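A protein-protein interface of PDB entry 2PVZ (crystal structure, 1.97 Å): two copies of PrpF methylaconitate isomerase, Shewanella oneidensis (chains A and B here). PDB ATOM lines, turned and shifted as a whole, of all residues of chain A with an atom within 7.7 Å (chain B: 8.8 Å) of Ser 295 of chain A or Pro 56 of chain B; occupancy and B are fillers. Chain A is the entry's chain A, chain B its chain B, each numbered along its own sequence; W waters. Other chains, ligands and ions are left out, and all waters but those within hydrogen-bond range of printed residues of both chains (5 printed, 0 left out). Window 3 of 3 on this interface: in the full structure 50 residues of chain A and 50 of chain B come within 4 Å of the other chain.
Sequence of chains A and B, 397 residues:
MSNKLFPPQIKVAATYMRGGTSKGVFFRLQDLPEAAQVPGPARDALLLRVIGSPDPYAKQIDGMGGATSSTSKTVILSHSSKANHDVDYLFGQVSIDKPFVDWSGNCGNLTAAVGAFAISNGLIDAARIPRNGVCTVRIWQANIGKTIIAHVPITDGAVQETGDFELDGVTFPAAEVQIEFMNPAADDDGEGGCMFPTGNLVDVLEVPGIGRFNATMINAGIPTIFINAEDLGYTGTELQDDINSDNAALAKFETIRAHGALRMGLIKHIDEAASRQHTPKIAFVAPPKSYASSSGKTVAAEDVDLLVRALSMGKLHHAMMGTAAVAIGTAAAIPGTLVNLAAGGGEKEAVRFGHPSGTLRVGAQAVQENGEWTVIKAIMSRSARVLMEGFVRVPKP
The backbone NH of Gly 169 of chain A lies within hydrogen-bond range of the side-chain hydroxyl of Tyr 57 of chain B (3.0 Å).
OG1 of Thr 171 of chain A lies within hydrogen-bond range of OD1 of Asp 55 of chain B (2.8 Å).
The backbone carbonyl oxygen (O) of Ser 294 of chain A lies close to the backbone carbonyl oxygen (O) of Pro 56 of chain B (3.4 Å).
N of Ser 294 of chain A is in hydrogen-bond range of O of Pro 356 of chain A (2.9 Å).
The side-chain hydroxyl of Ser 294 of chain A lies within hydrogen-bond range of the side-chain hydroxyl of Ser 357 of chain A.
The backbone carbonyl oxygen (O) of Ile 96 of chain B lies within hydrogen-bond range of the side-chain hydroxyl (OG) of Ser 53 of chain B.
N of Ala 58 of chain B sits at hydrogen-bond distance from OD2 of Asp 55 of chain B (3.3 Å).
OD2 of Asp 55 of chain B lies within hydrogen-bond range of N of Gln 60 of chain B.
O of Ile 96 of chain B is in hydrogen-bond range of N of Asp 55 of chain B, at 2.8 Å.
Among the printed residues, merely in contact across the chains: Thr 171 of chain A with Pro 54 of chain B, Ser 295 of chain A with Pro 56 of chain B, Ser 357 of chain A with Tyr 57 of chain B, Phe 172 of chain A with Ser 53 of chain B, Ser 294 of chain A with Tyr 57 of chain B, Ser 295 of chain A with Tyr 57 of chain B, Asp 168 of chain A with Tyr 57 of chain B, Val 170 of chain A with Tyr 57 of chain B and Phe 172 of chain A with Pro 54 of chain B.
Of the printed residues of chain B, Asp 168 of chain A touches Tyr 57.
Of the printed residues of chain B, Gly 169 of chain A touches Tyr 57.
Of the printed residues of chain B, Val 170 of chain A touches Tyr 57 (3.9 Å).
Of the printed residues of chain B, Ser 294 of chain A touches Pro 56 and Tyr 57.
Ser 295 of chain A touches two residues of chain B.
Val 299 of chain A touches none of the printed residues of chain B.
Of chain A, only Ser 294 and Ser 295 come within 4 Å of Pro 56 of chain B.
Printed residues of chain A within 4 Å of Tyr 57 of chain B: Asp 168 (3.7 Å), Gly 169 (3.0 Å), Val 170 (3.9 Å), Ser 294 (3.6 Å), Ser 295 (3.7 Å) and Ser 357 (3.5 Å).
Ser 95 of chain B touches none of the printed residues of chain A.
The nearest printed residue of chain B that does not touch Thr 171 of chain A is Tyr 57 of chain B (4.1 Å).
Hydrophobic or aromatic side chains of chain B that line the printed part of chain A: Pro 56 and Tyr 57.
Of the 17 printed residues of chain A, 8 touch a printed residue of chain B.
Among the printed residues, 12 pairs touch across the chains.
No position is printed for both chains.
Of the 12 pairs that touch across the chains among the printed residues, none has its exchanged pair printed and touching as well.
Water W3 lies within hydrogen-bond range of the side-chain hydroxyl of Tyr 57 of chain B (2.6 Å) and the backbone carbonyl oxygen of Val 170 of chain A (2.8 Å).
Water W2 lies within hydrogen-bond range of OD2 of Asp 55 of chain B (2.7 Å), OG1 of Thr 171 of chain A (3.4 Å) and N of Gln 60 of chain B (3.4 Å).
Water W4 lies within hydrogen-bond range of the side-chain hydroxyl (OG) of Ser 295 of chain A (2.7 Å) and the side-chain hydroxyl (OH) of Tyr 57 of chain B (2.9 Å).
Water W5 lies within hydrogen-bond range of the side-chain hydroxyl of Thr 171 of chain A (2.7 Å) and the backbone carbonyl oxygen of Gly 52 of chain B (2.8 Å).
Water W1 lies within hydrogen-bond range of the backbone carbonyl oxygen of Tyr 57 of chain B (2.8 Å) and the side-chain hydroxyl of Ser 294 of chain A (3.0 Å).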
ATOM      1  N   ASP A 168      10.676 -11.214  27.437  1.00  0.00           N
ATOM      2  CA  ASP A 168      10.628 -12.165  26.335  1.00  0.00           C
ATOM      3  C   ASP A 168      11.018 -11.471  25.030  1.00  0.00           C
ATOM      4  O   ASP A 168      10.443 -10.443  24.659  1.00  0.00           O
ATOM      5  CB  ASP A 168       9.251 -12.828  26.244  1.00  0.00           C
ATOM      6  CG  ASP A 168       9.017 -13.847  27.356  1.00  0.00           C
ATOM      7  OD1 ASP A 168       9.981 -14.211  28.070  1.00  0.00           O
ATOM      8  OD2 ASP A 168       7.866 -14.304  27.513  1.00  0.00           O
ATOM      9  N   GLY A 169      12.023 -12.020  24.360  1.00  0.00           N
ATOM     10  CA  GLY A 169      12.539 -11.430  23.131  1.00  0.00           C
ATOM     11  C   GLY A 169      13.856 -10.706  23.340  1.00  0.00           C
ATOM     12  O   GLY A 169      14.499 -10.292  22.375  1.00  0.00           O
ATOM     13  N   VAL A 170      14.247 -10.541  24.602  1.00  0.00           N
ATOM     14  CA  VAL A 170      15.543  -9.965  24.948  1.00  0.00           C
ATOM     15  C   VAL A 170      16.411 -11.060  25.548  1.00  0.00           C
ATOM     16  O   VAL A 170      16.073 -11.636  26.585  1.00  0.00           O
ATOM     17  CB  VAL A 170      15.415  -8.782  25.929  1.00  0.00           C
ATOM     18  CG1 VAL A 170      16.802  -8.231  26.279  1.00  0.00           C
ATOM     19  CG2 VAL A 170      14.535  -7.681  25.333  1.00  0.00           C
ATOM     20  N   THR A 171      17.527 -11.344  24.885  1.00  0.00           N
ATOM     21  CA  THR A 171      18.373 -12.483  25.234  1.00  0.00           C
ATOM     22  C   THR A 171      18.843 -12.473  26.703  1.00  0.00           C
ATOM     23  O   THR A 171      18.744 -13.480  27.402  1.00  0.00           O
ATOM     24  CB  THR A 171      19.596 -12.580  24.286  1.00  0.00           C
ATOM     25  OG1 THR A 171      19.160 -12.491  22.925  1.00  0.00           O
ATOM     26  CG2 THR A 171      20.326 -13.901  24.482  1.00  0.00           C
ATOM     27  N   PHE A 172      19.335 -11.329  27.161  1.00  0.00           N
ATOM     28  CA  PHE A 172      19.948 -11.251  28.471  1.00  0.00           C
ATOM     29  C   PHE A 172      19.220 -10.268  29.368  1.00  0.00           C
ATOM     30  O   PHE A 172      18.670  -9.277  28.883  1.00  0.00           O
ATOM     31  CB  PHE A 172      21.431 -10.875  28.351  1.00  0.00           C
ATOM     32  CG  PHE A 172      22.224 -11.826  27.498  1.00  0.00           C
ATOM     33  CD1 PHE A 172      22.562 -13.093  27.973  1.00  0.00           C
ATOM     34  CD2 PHE A 172      22.628 -11.458  26.222  1.00  0.00           C
ATOM     35  CE1 PHE A 172      23.290 -13.978  27.184  1.00  0.00           C
ATOM     36  CE2 PHE A 172      23.355 -12.343  25.416  1.00  0.00           C
ATOM     37  CZ  PHE A 172      23.686 -13.598  25.900  1.00  0.00           C
ATOM     38  N   LEU A 239       4.381 -18.565  14.116  1.00  0.00           N
ATOM     39  CA  LEU A 239       5.721 -18.014  14.219  1.00  0.00           C
ATOM     40  C   LEU A 239       6.115 -17.446  12.851  1.00  0.00           C
ATOM     41  O   LEU A 239       5.382 -17.607  11.871  1.00  0.00           O
ATOM     42  CB  LEU A 239       6.709 -19.086  14.703  1.00  0.00           C
ATOM     43  CG  LEU A 239       6.451 -19.721  16.082  1.00  0.00           C
ATOM     44  CD1 LEU A 239       7.509 -20.767  16.388  1.00  0.00           C
ATOM     45  CD2 LEU A 239       6.385 -18.676  17.208  1.00  0.00           C
ATOM     46  N   ALA A 292       4.671 -23.212  21.420  1.00  0.00           N
ATOM     47  CA  ALA A 292       6.104 -23.034  21.619  1.00  0.00           C
ATOM     48  C   ALA A 292       6.509 -21.687  21.000  1.00  0.00           C
ATOM     49  O   ALA A 292       6.184 -21.399  19.848  1.00  0.00           O
ATOM     50  CB  ALA A 292       6.869 -24.190  20.979  1.00  0.00           C
ATOM     51  N   SER A 293       7.183 -20.850  21.780  1.00  0.00           N
ATOM     52  CA  SER A 293       7.683 -19.579  21.275  1.00  0.00           C
ATOM     53  C   SER A 293       8.872 -19.820  20.347  1.00  0.00           C
ATOM     54  O   SER A 293       9.336 -20.954  20.201  1.00  0.00           O
ATOM     55  CB  SER A 293       8.109 -18.679  22.434  1.00  0.00           C
ATOM     56  OG  SER A 293       9.370 -19.087  22.926  1.00  0.00           O
ATOM     57  N   SER A 294       9.362 -18.745  19.731  1.00  0.00           N
ATOM     58  CA  SER A 294      10.547 -18.806  18.880  1.00  0.00           C
ATOM     59  C   SER A 294      11.805 -19.293  19.613  1.00  0.00           C
ATOM     60  O   SER A 294      12.748 -19.755  18.969  1.00  0.00           O
ATOM     61  CB  SER A 294      10.822 -17.436  18.268  1.00  0.00           C
ATOM     62  OG  SER A 294      11.013 -16.477  19.293  1.00  0.00           O
ATOM     63  N   SER A 295      11.829 -19.160  20.941  1.00  0.00           N
ATOM     64  CA  SER A 295      12.947 -19.665  21.759  1.00  0.00           C
ATOM     65  C   SER A 295      12.814 -21.149  22.135  1.00  0.00           C
ATOM     66  O   SER A 295      13.768 -21.757  22.631  1.00  0.00           O
ATOM     67  CB  SER A 295      13.115 -18.820  23.024  1.00  0.00           C
ATOM     68  OG  SER A 295      11.995 -18.950  23.886  1.00  0.00           O
ATOM     69  N   GLY A 296      11.641 -21.728  21.891  1.00  0.00           N
ATOM     70  CA  GLY A 296      11.365 -23.112  22.266  1.00  0.00           C
ATOM     71  C   GLY A 296      10.658 -23.230  23.604  1.00  0.00           C
ATOM     72  O   GLY A 296      10.292 -24.330  24.024  1.00  0.00           O
ATOM     73  N   LYS A 297      10.467 -22.097  24.275  1.00  0.00           N
ATOM     74  CA  LYS A 297       9.764 -22.043  25.550  1.00  0.00           C
ATOM     75  C   LYS A 297       8.250 -22.117  25.333  1.00  0.00           C
ATOM     76  O   LYS A 297       7.709 -21.447  24.449  1.00  0.00           O
ATOM     77  CB  LYS A 297      10.129 -20.757  26.303  1.00  0.00           C
ATOM     78  CG  LYS A 297       9.535 -20.662  27.703  1.00  0.00           C
ATOM     79  CD  LYS A 297      10.075 -19.470  28.478  1.00  0.00           C
ATOM     80  CE  LYS A 297       9.673 -19.538  29.950  1.00  0.00           C
ATOM     81  NZ  LYS A 297      10.621 -20.364  30.766  1.00  0.00           N
ATOM     82  N   THR A 298       7.575 -22.923  26.150  1.00  0.00           N
ATOM     83  CA  THR A 298       6.118 -23.035  26.092  1.00  0.00           C
ATOM     84  C   THR A 298       5.437 -21.799  26.667  1.00  0.00           C
ATOM     85  O   THR A 298       5.739 -21.369  27.778  1.00  0.00           O
ATOM     86  CB  THR A 298       5.614 -24.302  26.828  1.00  0.00           C
ATOM     87  OG1 THR A 298       6.147 -25.462  26.181  1.00  0.00           O
ATOM     88  CG2 THR A 298       4.081 -24.378  26.824  1.00  0.00           C
ATOM     89  N   VAL A 299       4.530 -21.223  25.881  1.00  0.00           N
ATOM     90  CA  VAL A 299       3.616 -20.213  26.371  1.00  0.00           C
ATOM     91  C   VAL A 299       2.272 -20.914  26.594  1.00  0.00           C
ATOM     92  O   VAL A 299       1.591 -21.268  25.646  1.00  0.00           O
ATOM     93  CB  VAL A 299       3.472 -19.031  25.377  1.00  0.00           C
ATOM     94  CG1 VAL A 299       2.491 -17.986  25.907  1.00  0.00           C
ATOM     95  CG2 VAL A 299       4.837 -18.389  25.096  1.00  0.00           C
ATOM     96  N   PRO A 356       5.104 -13.961  19.069  1.00  0.00           N
ATOM     97  CA  PRO A 356       5.982 -15.078  18.691  1.00  0.00           C
ATOM     98  C   PRO A 356       7.125 -15.394  19.665  1.00  0.00           C
ATOM     99  O   PRO A 356       7.550 -16.542  19.740  1.00  0.00           O
ATOM    100  CB  PRO A 356       6.536 -14.641  17.331  1.00  0.00           C
ATOM    101  CG  PRO A 356       5.439 -13.787  16.767  1.00  0.00           C
ATOM    102  CD  PRO A 356       4.966 -12.995  17.961  1.00  0.00           C
ATOM    103  N   SER A 357       7.607 -14.395  20.401  1.00  0.00           N
ATOM    104  CA  SER A 357       8.781 -14.575  21.267  1.00  0.00           C
ATOM    105  C   SER A 357       8.455 -14.863  22.733  1.00  0.00           C
ATOM    106  O   SER A 357       9.362 -15.079  23.535  1.00  0.00           O
ATOM    107  CB  SER A 357       9.722 -13.366  21.170  1.00  0.00           C
ATOM    108  OG  SER A 357      10.421 -13.388  19.945  1.00  0.00           O
ATOM    109  N   GLY A 358       7.170 -14.873  23.078  1.00  0.00           N
ATOM    110  CA  GLY A 358       6.758 -15.048  24.463  1.00  0.00           C
ATOM    111  C   GLY A 358       5.603 -14.137  24.812  1.00  0.00           C
ATOM    112  O   GLY A 358       4.666 -13.979  24.023  1.00  0.00           O
ATOM    113  N   GLY B  52      26.231 -11.089  21.013  1.00  0.00           N
ATOM    114  CA  GLY B  52      24.847 -11.315  21.446  1.00  0.00           C
ATOM    115  C   GLY B  52      24.447 -12.780  21.483  1.00  0.00           C
ATOM    116  O   GLY B  52      23.260 -13.106  21.355  1.00  0.00           O
ATOM    117  N   SER B  53      25.443 -13.654  21.649  1.00  0.00           N
ATOM    118  CA  SER B  53      25.260 -15.116  21.659  1.00  0.00           C
ATOM    119  C   SER B  53      25.558 -15.705  23.045  1.00  0.00           C
ATOM    120  O   SER B  53      26.229 -15.060  23.845  1.00  0.00           O
ATOM    121  CB  SER B  53      26.196 -15.762  20.624  1.00  0.00           C
ATOM    122  OG  SER B  53      25.737 -15.532  19.302  1.00  0.00           O
ATOM    123  N   PRO B  54      25.036 -16.914  23.351  1.00  0.00           N
ATOM    124  CA  PRO B  54      24.094 -17.697  22.542  1.00  0.00           C
ATOM    125  C   PRO B  54      22.713 -17.053  22.605  1.00  0.00           C
ATOM    126  O   PRO B  54      22.336 -16.504  23.649  1.00  0.00           O
ATOM    127  CB  PRO B  54      24.070 -19.055  23.244  1.00  0.00           C
ATOM    128  CG  PRO B  54      24.395 -18.751  24.663  1.00  0.00           C
ATOM    129  CD  PRO B  54      25.376 -17.601  24.613  1.00  0.00           C
ATOM    130  N   ASP B  55      21.985 -17.096  21.491  1.00  0.00           N
ATOM    131  CA  ASP B  55      20.677 -16.464  21.421  1.00  0.00           C
ATOM    132  C   ASP B  55      19.608 -17.455  20.979  1.00  0.00           C
ATOM    133  O   ASP B  55      19.550 -17.812  19.800  1.00  0.00           O
ATOM    134  CB  ASP B  55      20.697 -15.261  20.469  1.00  0.00           C
ATOM    135  CG  ASP B  55      19.363 -14.540  20.421  1.00  0.00           C
ATOM    136  OD1 ASP B  55      18.567 -14.700  21.375  1.00  0.00           O
ATOM    137  OD2 ASP B  55      19.107 -13.803  19.442  1.00  0.00           O
ATOM    138  N   PRO B  56      18.746 -17.892  21.915  1.00  0.00           N
ATOM    139  CA  PRO B  56      17.687 -18.840  21.533  1.00  0.00           C
ATOM    140  C   PRO B  56      16.638 -18.237  20.596  1.00  0.00           C
ATOM    141  O   PRO B  56      15.890 -18.981  19.951  1.00  0.00           O
ATOM    142  CB  PRO B  56      17.073 -19.259  22.876  1.00  0.00           C
ATOM    143  CG  PRO B  56      17.446 -18.177  23.835  1.00  0.00           C
ATOM    144  CD  PRO B  56      18.719 -17.558  23.349  1.00  0.00           C
ATOM    145  N   TYR B  57      16.587 -16.906  20.504  1.00  0.00           N
ATOM    146  CA  TYR B  57      15.683 -16.237  19.555  1.00  0.00           C
ATOM    147  C   TYR B  57      16.268 -16.150  18.144  1.00  0.00           C
ATOM    148  O   TYR B  57      15.544 -15.876  17.189  1.00  0.00           O
ATOM    149  CB  TYR B  57      15.321 -14.826  20.038  1.00  0.00           C
ATOM    150  CG  TYR B  57      14.718 -14.785  21.426  1.00  0.00           C
ATOM    151  CD1 TYR B  57      15.461 -14.310  22.512  1.00  0.00           C
ATOM    152  CD2 TYR B  57      13.412 -15.218  21.651  1.00  0.00           C
ATOM    153  CE1 TYR B  57      14.915 -14.266  23.787  1.00  0.00           C
ATOM    154  CE2 TYR B  57      12.855 -15.177  22.924  1.00  0.00           C
ATOM    155  CZ  TYR B  57      13.613 -14.704  23.984  1.00  0.00           C
ATOM    156  OH  TYR B  57      13.068 -14.666  25.249  1.00  0.00           O
ATOM    157  N   ALA B  58      17.582 -16.363  18.037  1.00  0.00           N
ATOM    158  CA  ALA B  58      18.319 -16.325  16.759  1.00  0.00           C
ATOM    159  C   ALA B  58      18.168 -14.999  15.999  1.00  0.00           C
ATOM    160  O   ALA B  58      18.026 -14.988  14.769  1.00  0.00           O
ATOM    161  CB  ALA B  58      17.936 -17.509  15.872  1.00  0.00           C
ATOM    162  N   LYS B  59      18.211 -13.894  16.750  1.00  0.00           N
ATOM    163  CA  LYS B  59      18.072 -12.538  16.196  1.00  0.00           C
ATOM    164  C   LYS B  59      19.262 -11.625  16.518  1.00  0.00           C
ATOM    165  O   LYS B  59      19.462 -10.601  15.848  1.00  0.00           O
ATOM    166  CB  LYS B  59      16.770 -11.884  16.691  1.00  0.00           C
ATOM    167  CG  LYS B  59      15.480 -12.571  16.199  1.00  0.00           C
ATOM    168  CD  LYS B  59      15.428 -12.658  14.664  1.00  0.00           C
ATOM    169  CE  LYS B  59      14.236 -13.483  14.181  1.00  0.00           C
ATOM    170  NZ  LYS B  59      14.143 -13.528  12.690  1.00  0.00           N
ATOM    171  N   GLN B  60      20.039 -11.995  17.537  1.00  0.00           N
ATOM    172  CA  GLN B  60      21.179 -11.196  18.026  1.00  0.00           C
ATOM    173  C   GLN B  60      20.842  -9.710  18.233  1.00  0.00           C
ATOM    174  O   GLN B  60      21.601  -8.812  17.866  1.00  0.00           O
ATOM    175  CB  GLN B  60      22.424 -11.406  17.153  1.00  0.00           C
ATOM    176  CG  GLN B  60      23.059 -12.776  17.390  1.00  0.00           C
ATOM    177  CD  GLN B  60      24.203 -13.099  16.445  1.00  0.00           C
ATOM    178  OE1 GLN B  60      24.264 -12.608  15.313  1.00  0.00           O
ATOM    179  NE2 GLN B  60      25.115 -13.950  16.906  1.00  0.00           N
ATOM    180  N   SER B  95      29.040 -18.716  17.066  1.00  0.00           N
ATOM    181  CA  SER B  95      27.778 -19.429  16.891  1.00  0.00           C
ATOM    182  C   SER B  95      26.619 -18.550  17.344  1.00  0.00           C
ATOM    183  O   SER B  95      26.720 -17.860  18.350  1.00  0.00           O
ATOM    184  CB  SER B  95      27.779 -20.740  17.685  1.00  0.00           C
ATOM    185  OG  SER B  95      26.490 -21.328  17.667  1.00  0.00           O
ATOM    186  N   ILE B  96      25.520 -18.589  16.594  1.00  0.00           N
ATOM    187  CA  ILE B  96      24.339 -17.787  16.920  1.00  0.00           C
ATOM    188  C   ILE B  96      23.550 -18.421  18.078  1.00  0.00           C
ATOM    189  O   ILE B  96      23.053 -17.719  18.965  1.00  0.00           O
ATOM    190  CB  ILE B  96      23.435 -17.596  15.674  1.00  0.00           C
ATOM    191  CG1 ILE B  96      24.176 -16.767  14.603  1.00  0.00           C
ATOM    192  CG2 ILE B  96      22.073 -16.967  16.053  1.00  0.00           C
ATOM    193  CD1 ILE B  96      23.612 -16.917  13.186  1.00  0.00           C
ATOM    194  N   ASP B  97      23.466 -19.746  18.065  1.00  0.00           N
ATOM    195  CA  ASP B  97      22.584 -20.492  18.963  1.00  0.00           C
ATOM    196  C   ASP B  97      23.299 -21.193  20.129  1.00  0.00           C
ATOM    197  O   ASP B  97      22.659 -21.547  21.118  1.00  0.00           O
ATOM    198  CB  ASP B  97      21.776 -21.514  18.151  1.00  0.00           C
ATOM    199  CG  ASP B  97      22.656 -22.512  17.418  1.00  0.00           C
ATOM    200  OD1 ASP B  97      23.612 -22.099  16.730  1.00  0.00           O
ATOM    201  OD2 ASP B  97      22.389 -23.726  17.518  1.00  0.00           O
ATOM    202  N   LYS B  98      24.611 -21.391  20.014  1.00  0.00           N
ATOM    203  CA  LYS B  98      25.379 -22.134  21.021  1.00  0.00           C
ATOM    204  C   LYS B  98      26.441 -21.254  21.669  1.00  0.00           C
ATOM    205  O   LYS B  98      26.941 -20.339  21.027  1.00  0.00           O
ATOM    206  CB  LYS B  98      26.047 -23.356  20.384  1.00  0.00           C
ATOM    207  CG  LYS B  98      25.074 -24.331  19.748  1.00  0.00           C
ATOM    208  CD  LYS B  98      25.817 -25.399  18.971  1.00  0.00           C
HETATM  209  O   HOH W   1      12.871 -14.978  17.431  1.00  0.00           O
HETATM  210  O   HOH W   2      17.780 -11.521  20.010  1.00  0.00           O
HETATM  211  O   HOH W   3      14.639 -13.927  27.182  1.00  0.00           O
HETATM  212  O   HOH W   4      12.194 -17.284  26.020  1.00  0.00           O
HETATM  213  O   HOH W   5      21.085 -11.325  21.403  1.00  0.00           O
